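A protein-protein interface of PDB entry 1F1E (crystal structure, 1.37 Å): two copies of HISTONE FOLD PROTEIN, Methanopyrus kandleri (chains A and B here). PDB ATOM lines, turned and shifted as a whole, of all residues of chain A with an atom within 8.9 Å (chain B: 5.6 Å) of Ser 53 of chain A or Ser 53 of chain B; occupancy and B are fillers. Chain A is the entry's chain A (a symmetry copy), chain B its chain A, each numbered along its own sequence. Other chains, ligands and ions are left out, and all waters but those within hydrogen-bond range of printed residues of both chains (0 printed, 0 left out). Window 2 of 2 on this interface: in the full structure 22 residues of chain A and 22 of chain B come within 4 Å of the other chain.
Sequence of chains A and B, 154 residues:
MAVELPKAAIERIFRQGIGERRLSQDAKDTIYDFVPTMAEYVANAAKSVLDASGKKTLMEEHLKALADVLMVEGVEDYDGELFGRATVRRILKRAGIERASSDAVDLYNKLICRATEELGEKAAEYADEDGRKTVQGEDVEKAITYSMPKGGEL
A ring nitrogen (NE2) of His 62 of chain A sits at hydrogen-bond distance from the backbone carbonyl oxygen of Ala 52 of chain B (3.4 Å). The backbone carbonyl oxygen (O) of Ala 52 of chain A lies within hydrogen-bond range of a ring nitrogen (NE2) of His 62 of chain B (3.4 Å). The backbone carbonyl oxygen (O) of Ser 53 of chain B sits close to the backbone carbonyl oxygen (O) of Ser 53 of chain A, 2.9 Å away.
OG of Ser 53 of chain B is in hydrogen-bond range of O of Leu 50 of chain B (2.7 Å). The side-chain hydroxyl (OG) of Ser 53 of chain B sits close to the backbone NH (N) of Lys 55 of chain B, 3.2 Å away. O of Leu 50 of chain A is in hydrogen-bond range of OG of Ser 53 of chain A, at 2.7 Å. The side-chain hydroxyl of Ser 53 of chain A lies close to the backbone NH of Lys 55 of chain A (3.2 Å). N of Met 59 of chain A lies within hydrogen-bond range of ND1 of His 62 of chain A, 3.3 Å away.
Ala 52 of chain B touches Glu 61 of chain A (CB to O, 3.1 Å). Ala 65 of chain A touches Ser 48 of chain B.
Printed residues of chain B within 4 Å of Ser 53 of chain A: Ser 53. Printed residues of chain A within 4 Å of Ser 53 of chain B: Ser 53 (2.9 Å). Of the printed residues of chain B, Glu 61 of chain A touches Ala 52 (3.1 Å). Of the printed residues of chain B, Ala 65 of chain A touches Ser 48. Thr 57 of chain A touches none of the printed residues of chain B. The nearest printed residue of chain B that does not touch Ser 53 of chain A is His 62 of chain B (4.8 Å). The nearest printed residue of chain A that does not touch Ser 53 of chain B is His 62 of chain A (4.8 Å).
Of the 9 printed residues of chain B, 4 touch a printed residue of chain A. Printed residues of chain B that touch a printed residue of chain A: Ser 48, Ala 52, Ser 53 and His 62. Among the printed residues, 5 pairs touch across the chains. Among the printed residues, no Asp or Glu carboxylate lies within 4 Å of a Lys or Arg side-chain nitrogen of the other chain.
Ala 52 of chain A touches His 62 of chain B, and with the chains exchanged His 62 of chain A touches Ala 52 of chain B. Ser 53 of chain B touches its own counterpart, Ser 53 of chain A. 9 positions are printed for both chains.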
ATOM      1  N   ALA A  46      -9.462  16.563  23.524  1.00  0.00           N
ATOM      2  CA  ALA A  46      -9.934  16.970  22.222  1.00  0.00           C
ATOM      3  C   ALA A  46     -11.419  17.310  22.271  1.00  0.00           C
ATOM      4  O   ALA A  46     -11.758  18.343  21.684  1.00  0.00           O
ATOM      5  CB  ALA A  46      -9.669  15.853  21.224  1.00  0.00           C
ATOM      6  N   LYS A  47     -12.214  16.519  22.966  1.00  0.00           N
ATOM      7  CA  LYS A  47     -13.627  16.878  23.086  1.00  0.00           C
ATOM      8  C   LYS A  47     -13.776  18.213  23.830  1.00  0.00           C
ATOM      9  O   LYS A  47     -14.570  19.075  23.415  1.00  0.00           O
ATOM     10  CB  LYS A  47     -14.390  15.769  23.778  1.00  0.00           C
ATOM     11  CG  LYS A  47     -15.836  16.034  24.128  1.00  0.00           C
ATOM     12  CD  LYS A  47     -16.753  16.243  22.930  1.00  0.00           C
ATOM     13  CE  LYS A  47     -18.208  16.208  23.410  1.00  0.00           C
ATOM     14  NZ  LYS A  47     -19.060  16.610  22.265  1.00  0.00           N
ATOM     15  N   SER A  48     -13.027  18.410  24.911  1.00  0.00           N
ATOM     16  CA  SER A  48     -13.073  19.649  25.674  1.00  0.00           C
ATOM     17  C   SER A  48     -12.729  20.819  24.759  1.00  0.00           C
ATOM     18  O   SER A  48     -13.458  21.843  24.822  1.00  0.00           O
ATOM     19  CB  SER A  48     -12.116  19.607  26.846  1.00  0.00           C
ATOM     20  OG  SER A  48     -12.497  18.611  27.778  1.00  0.00           O
ATOM     21  N   VAL A  49     -11.701  20.729  23.940  1.00  0.00           N
ATOM     22  CA  VAL A  49     -11.306  21.827  23.050  1.00  0.00           C
ATOM     23  C   VAL A  49     -12.373  22.029  21.997  1.00  0.00           C
ATOM     24  O   VAL A  49     -12.675  23.197  21.672  1.00  0.00           O
ATOM     25  CB  VAL A  49      -9.906  21.554  22.497  1.00  0.00           C
ATOM     26  CG1 VAL A  49      -9.532  22.566  21.433  1.00  0.00           C
ATOM     27  CG2 VAL A  49      -8.913  21.515  23.661  1.00  0.00           C
ATOM     28  N   LEU A  50     -13.010  20.966  21.484  1.00  0.00           N
ATOM     29  CA  LEU A  50     -14.147  21.158  20.559  1.00  0.00           C
ATOM     30  C   LEU A  50     -15.458  21.547  21.217  1.00  0.00           C
ATOM     31  O   LEU A  50     -16.233  22.386  20.683  1.00  0.00           O
ATOM     32  CB  LEU A  50     -14.271  19.865  19.726  1.00  0.00           C
ATOM     33  CG  LEU A  50     -15.552  19.749  18.904  1.00  0.00           C
ATOM     34  CD1 LEU A  50     -15.461  20.571  17.629  1.00  0.00           C
ATOM     35  CD2 LEU A  50     -15.836  18.284  18.596  1.00  0.00           C
ATOM     36  N   ASP A  51     -15.932  21.054  22.355  1.00  0.00           N
ATOM     37  CA  ASP A  51     -17.172  21.619  22.889  1.00  0.00           C
ATOM     38  C   ASP A  51     -17.050  23.101  23.246  1.00  0.00           C
ATOM     39  O   ASP A  51     -17.987  23.858  23.032  1.00  0.00           O
ATOM     40  CB  ASP A  51     -17.600  20.874  24.148  1.00  0.00           C
ATOM     41  CG  ASP A  51     -18.277  19.553  23.832  1.00  0.00           C
ATOM     42  OD1 ASP A  51     -18.523  19.162  22.685  1.00  0.00           O
ATOM     43  OD2 ASP A  51     -18.549  18.906  24.848  1.00  0.00           O
ATOM     44  N   ALA A  52     -15.899  23.530  23.727  1.00  0.00           N
ATOM     45  CA  ALA A  52     -15.696  24.945  23.995  1.00  0.00           C
ATOM     46  C   ALA A  52     -15.710  25.744  22.709  1.00  0.00           C
ATOM     47  O   ALA A  52     -15.910  26.958  22.684  1.00  0.00           O
ATOM     48  CB  ALA A  52     -14.369  25.131  24.711  1.00  0.00           C
ATOM     49  N   SER A  53     -15.475  25.050  21.607  1.00  0.00           N
ATOM     50  CA  SER A  53     -15.195  25.767  20.376  1.00  0.00           C
ATOM     51  C   SER A  53     -16.429  26.168  19.578  1.00  0.00           C
ATOM     52  O   SER A  53     -16.252  26.849  18.564  1.00  0.00           O
ATOM     53  CB  SER A  53     -14.273  24.947  19.442  1.00  0.00           C
ATOM     54  OG  SER A  53     -15.040  23.905  18.855  1.00  0.00           O
ATOM     55  N   GLY A  54     -17.598  25.711  20.005  1.00  0.00           N
ATOM     56  CA  GLY A  54     -18.844  25.980  19.287  1.00  0.00           C
ATOM     57  C   GLY A  54     -18.979  25.142  18.031  1.00  0.00           C
ATOM     58  O   GLY A  54     -19.882  25.231  17.189  1.00  0.00           O
ATOM     59  N   LYS A  55     -18.073  24.201  17.786  1.00  0.00           N
ATOM     60  CA  LYS A  55     -18.303  23.341  16.598  1.00  0.00           C
ATOM     61  C   LYS A  55     -18.686  21.908  16.911  1.00  0.00           C
ATOM     62  O   LYS A  55     -18.388  21.471  18.041  1.00  0.00           O
ATOM     63  CB  LYS A  55     -16.981  23.433  15.882  1.00  0.00           C
ATOM     64  N   LYS A  56     -19.324  21.086  16.066  1.00  0.00           N
ATOM     65  CA  LYS A  56     -19.485  19.670  16.416  1.00  0.00           C
ATOM     66  C   LYS A  56     -18.504  18.772  15.713  1.00  0.00           C
ATOM     67  O   LYS A  56     -18.333  17.571  15.992  1.00  0.00           O
ATOM     68  CB  LYS A  56     -20.895  19.158  16.085  1.00  0.00           C
ATOM     69  N   THR A  57     -17.814  19.387  14.761  1.00  0.00           N
ATOM     70  CA  THR A  57     -16.836  18.569  14.035  1.00  0.00           C
ATOM     71  C   THR A  57     -15.416  18.848  14.524  1.00  0.00           C
ATOM     72  O   THR A  57     -14.926  19.951  14.470  1.00  0.00           O
ATOM     73  CB  THR A  57     -16.926  18.800  12.548  1.00  0.00           C
ATOM     74  OG1 THR A  57     -18.259  18.616  12.110  1.00  0.00           O
ATOM     75  CG2 THR A  57     -16.069  17.724  11.888  1.00  0.00           C
ATOM     76  N   LEU A  58     -14.785  17.756  14.952  1.00  0.00           N
ATOM     77  CA  LEU A  58     -13.367  17.846  15.333  1.00  0.00           C
ATOM     78  C   LEU A  58     -12.565  18.039  14.078  1.00  0.00           C
ATOM     79  O   LEU A  58     -12.730  17.350  13.070  1.00  0.00           O
ATOM     80  CB  LEU A  58     -12.905  16.555  16.012  1.00  0.00           C
ATOM     81  CG  LEU A  58     -11.558  16.586  16.738  1.00  0.00           C
ATOM     82  CD1 LEU A  58     -11.640  17.426  18.008  1.00  0.00           C
ATOM     83  CD2 LEU A  58     -11.113  15.172  17.074  1.00  0.00           C
ATOM     84  N   MET A  59     -11.673  18.980  13.974  1.00  0.00           N
ATOM     85  CA  MET A  59     -10.760  19.465  12.993  1.00  0.00           C
ATOM     86  C   MET A  59      -9.328  19.486  13.533  1.00  0.00           C
ATOM     87  O   MET A  59      -9.070  19.390  14.705  1.00  0.00           O
ATOM     88  CB  MET A  59     -11.168  20.802  12.422  1.00  0.00           C
ATOM     89  CG  MET A  59     -12.686  20.997  12.307  1.00  0.00           C
ATOM     90  SD  MET A  59     -13.338  20.239  10.818  1.00  0.00           S
ATOM     91  CE  MET A  59     -12.562  21.188   9.525  1.00  0.00           C
ATOM     92  N   GLU A  61      -7.273  21.778  13.782  1.00  0.00           N
ATOM     93  CA  GLU A  61      -6.885  22.915  14.639  1.00  0.00           C
ATOM     94  C   GLU A  61      -7.144  22.534  16.094  1.00  0.00           C
ATOM     95  O   GLU A  61      -6.472  22.967  17.006  1.00  0.00           O
ATOM     96  CB  GLU A  61      -7.576  24.238  14.311  1.00  0.00           C
ATOM     97  CG  GLU A  61      -7.819  24.578  12.846  1.00  0.00           C
ATOM     98  CD  GLU A  61      -8.819  23.656  12.153  1.00  0.00           C
ATOM     99  N   HIS A  62      -8.151  21.669  16.382  1.00  0.00           N
ATOM    100  CA  HIS A  62      -8.349  21.295  17.770  1.00  0.00           C
ATOM    101  C   HIS A  62      -7.203  20.446  18.343  1.00  0.00           C
ATOM    102  O   HIS A  62      -6.799  20.655  19.509  1.00  0.00           O
ATOM    103  CB  HIS A  62      -9.656  20.499  17.877  1.00  0.00           C
ATOM    104  CG  HIS A  62     -10.719  21.389  17.331  1.00  0.00           C
ATOM    105  ND1 HIS A  62     -11.766  20.855  16.682  1.00  0.00           N
ATOM    106  CD2 HIS A  62     -10.937  22.703  17.309  1.00  0.00           C
ATOM    107  CE1 HIS A  62     -12.611  21.769  16.257  1.00  0.00           C
ATOM    108  NE2 HIS A  62     -12.114  22.973  16.640  1.00  0.00           N
ATOM    109  N   ALA A  65      -4.111  22.609  18.899  1.00  0.00           N
ATOM    110  CA  ALA A  65      -4.142  23.264  20.212  1.00  0.00           C
ATOM    111  C   ALA A  65      -3.729  22.323  21.327  1.00  0.00           C
ATOM    112  O   ALA A  65      -2.962  22.757  22.176  1.00  0.00           O
ATOM    113  CB  ALA A  65      -5.527  23.832  20.485  1.00  0.00           C
ATOM    114  N   SER B  48      -4.374  29.363  22.051  1.00  0.00           N
ATOM    115  CA  SER B  48      -4.401  28.166  21.225  1.00  0.00           C
ATOM    116  C   SER B  48      -5.815  27.597  21.204  1.00  0.00           C
ATOM    117  O   SER B  48      -6.289  27.248  20.091  1.00  0.00           O
ATOM    118  CB  SER B  48      -3.430  27.124  21.737  1.00  0.00           C
ATOM    119  OG  SER B  48      -2.093  27.583  21.639  1.00  0.00           O
ATOM    120  N   VAL B  49      -6.494  27.491  22.329  1.00  0.00           N
ATOM    121  CA  VAL B  49      -7.851  26.933  22.378  1.00  0.00           C
ATOM    122  C   VAL B  49      -8.804  27.867  21.666  1.00  0.00           C
ATOM    123  O   VAL B  49      -9.697  27.369  20.947  1.00  0.00           O
ATOM    124  CB  VAL B  49      -8.220  26.627  23.831  1.00  0.00           C
ATOM    125  CG1 VAL B  49      -9.676  26.222  23.950  1.00  0.00           C
ATOM    126  CG2 VAL B  49      -7.259  25.567  24.375  1.00  0.00           C
ATOM    127  N   LEU B  50      -8.637  29.193  21.769  1.00  0.00           N
ATOM    128  CA  LEU B  50      -9.474  30.110  20.968  1.00  0.00           C
ATOM    129  C   LEU B  50      -9.082  30.238  19.508  1.00  0.00           C
ATOM    130  O   LEU B  50      -9.955  30.325  18.602  1.00  0.00           O
ATOM    131  CB  LEU B  50      -9.471  31.471  21.696  1.00  0.00           C
ATOM    132  CG  LEU B  50     -10.050  32.633  20.893  1.00  0.00           C
ATOM    133  CD1 LEU B  50     -11.570  32.613  20.920  1.00  0.00           C
ATOM    134  CD2 LEU B  50      -9.507  33.951  21.428  1.00  0.00           C
ATOM    135  N   ASP B  51      -7.841  30.300  19.040  1.00  0.00           N
ATOM    136  CA  ASP B  51      -7.650  30.324  17.589  1.00  0.00           C
ATOM    137  C   ASP B  51      -8.156  29.058  16.897  1.00  0.00           C
ATOM    138  O   ASP B  51      -8.710  29.139  15.809  1.00  0.00           O
ATOM    139  CB  ASP B  51      -6.174  30.479  17.247  1.00  0.00           C
ATOM    140  CG  ASP B  51      -5.699  31.915  17.386  1.00  0.00           C
ATOM    141  OD1 ASP B  51      -6.442  32.862  17.668  1.00  0.00           O
ATOM    142  OD2 ASP B  51      -4.486  32.033  17.192  1.00  0.00           O
ATOM    143  N   ALA B  52      -8.027  27.910  17.534  1.00  0.00           N
ATOM    144  CA  ALA B  52      -8.575  26.688  16.965  1.00  0.00           C
ATOM    145  C   ALA B  52     -10.087  26.747  16.918  1.00  0.00           C
ATOM    146  O   ALA B  52     -10.756  26.021  16.183  1.00  0.00           O
ATOM    147  CB  ALA B  52      -8.124  25.503  17.803  1.00  0.00           C
ATOM    148  N   SER B  53     -10.647  27.624  17.736  1.00  0.00           N
ATOM    149  CA  SER B  53     -12.080  27.554  17.960  1.00  0.00           C
ATOM    150  C   SER B  53     -12.921  28.319  16.945  1.00  0.00           C
ATOM    151  O   SER B  53     -14.147  28.228  17.043  1.00  0.00           O
ATOM    152  CB  SER B  53     -12.457  28.068  19.370  1.00  0.00           C
ATOM    153  OG  SER B  53     -12.358  29.485  19.374  1.00  0.00           O
ATOM    154  N   GLY B  54     -12.270  29.068  16.065  1.00  0.00           N
ATOM    155  CA  GLY B  54     -12.972  29.893  15.081  1.00  0.00           C
ATOM    156  C   GLY B  54     -13.569  31.142  15.698  1.00  0.00           C
ATOM    157  O   GLY B  54     -14.291  31.966  15.121  1.00  0.00           O
ATOM    158  N   LYS B  55     -13.301  31.424  16.969  1.00  0.00           N
ATOM    159  CA  LYS B  55     -13.826  32.708  17.498  1.00  0.00           C
ATOM    160  C   LYS B  55     -12.774  33.764  17.769  1.00  0.00           C
ATOM    161  O   LYS B  55     -11.599  33.374  17.926  1.00  0.00           O
ATOM    162  CB  LYS B  55     -14.527  32.267  18.755  1.00  0.00           C
ATOM    163  N   HIS B  62     -13.489  28.486  26.876  1.00  0.00           N
ATOM    164  CA  HIS B  62     -12.113  28.198  26.519  1.00  0.00           C
ATOM    165  C   HIS B  62     -11.216  27.899  27.730  1.00  0.00           C
ATOM    166  O   HIS B  62     -10.364  26.984  27.661  1.00  0.00           O
ATOM    167  CB  HIS B  62     -11.543  29.408  25.767  1.00  0.00           C
ATOM    168  CG  HIS B  62     -12.443  29.621  24.599  1.00  0.00           C
ATOM    169  ND1 HIS B  62     -12.660  30.865  24.143  1.00  0.00           N
ATOM    170  CD2 HIS B  62     -13.164  28.834  23.801  1.00  0.00           C
ATOM    171  CE1 HIS B  62     -13.479  30.887  23.114  1.00  0.00           C
ATOM    172  NE2 HIS B  62     -13.827  29.599  22.861  1.00  0.00           N
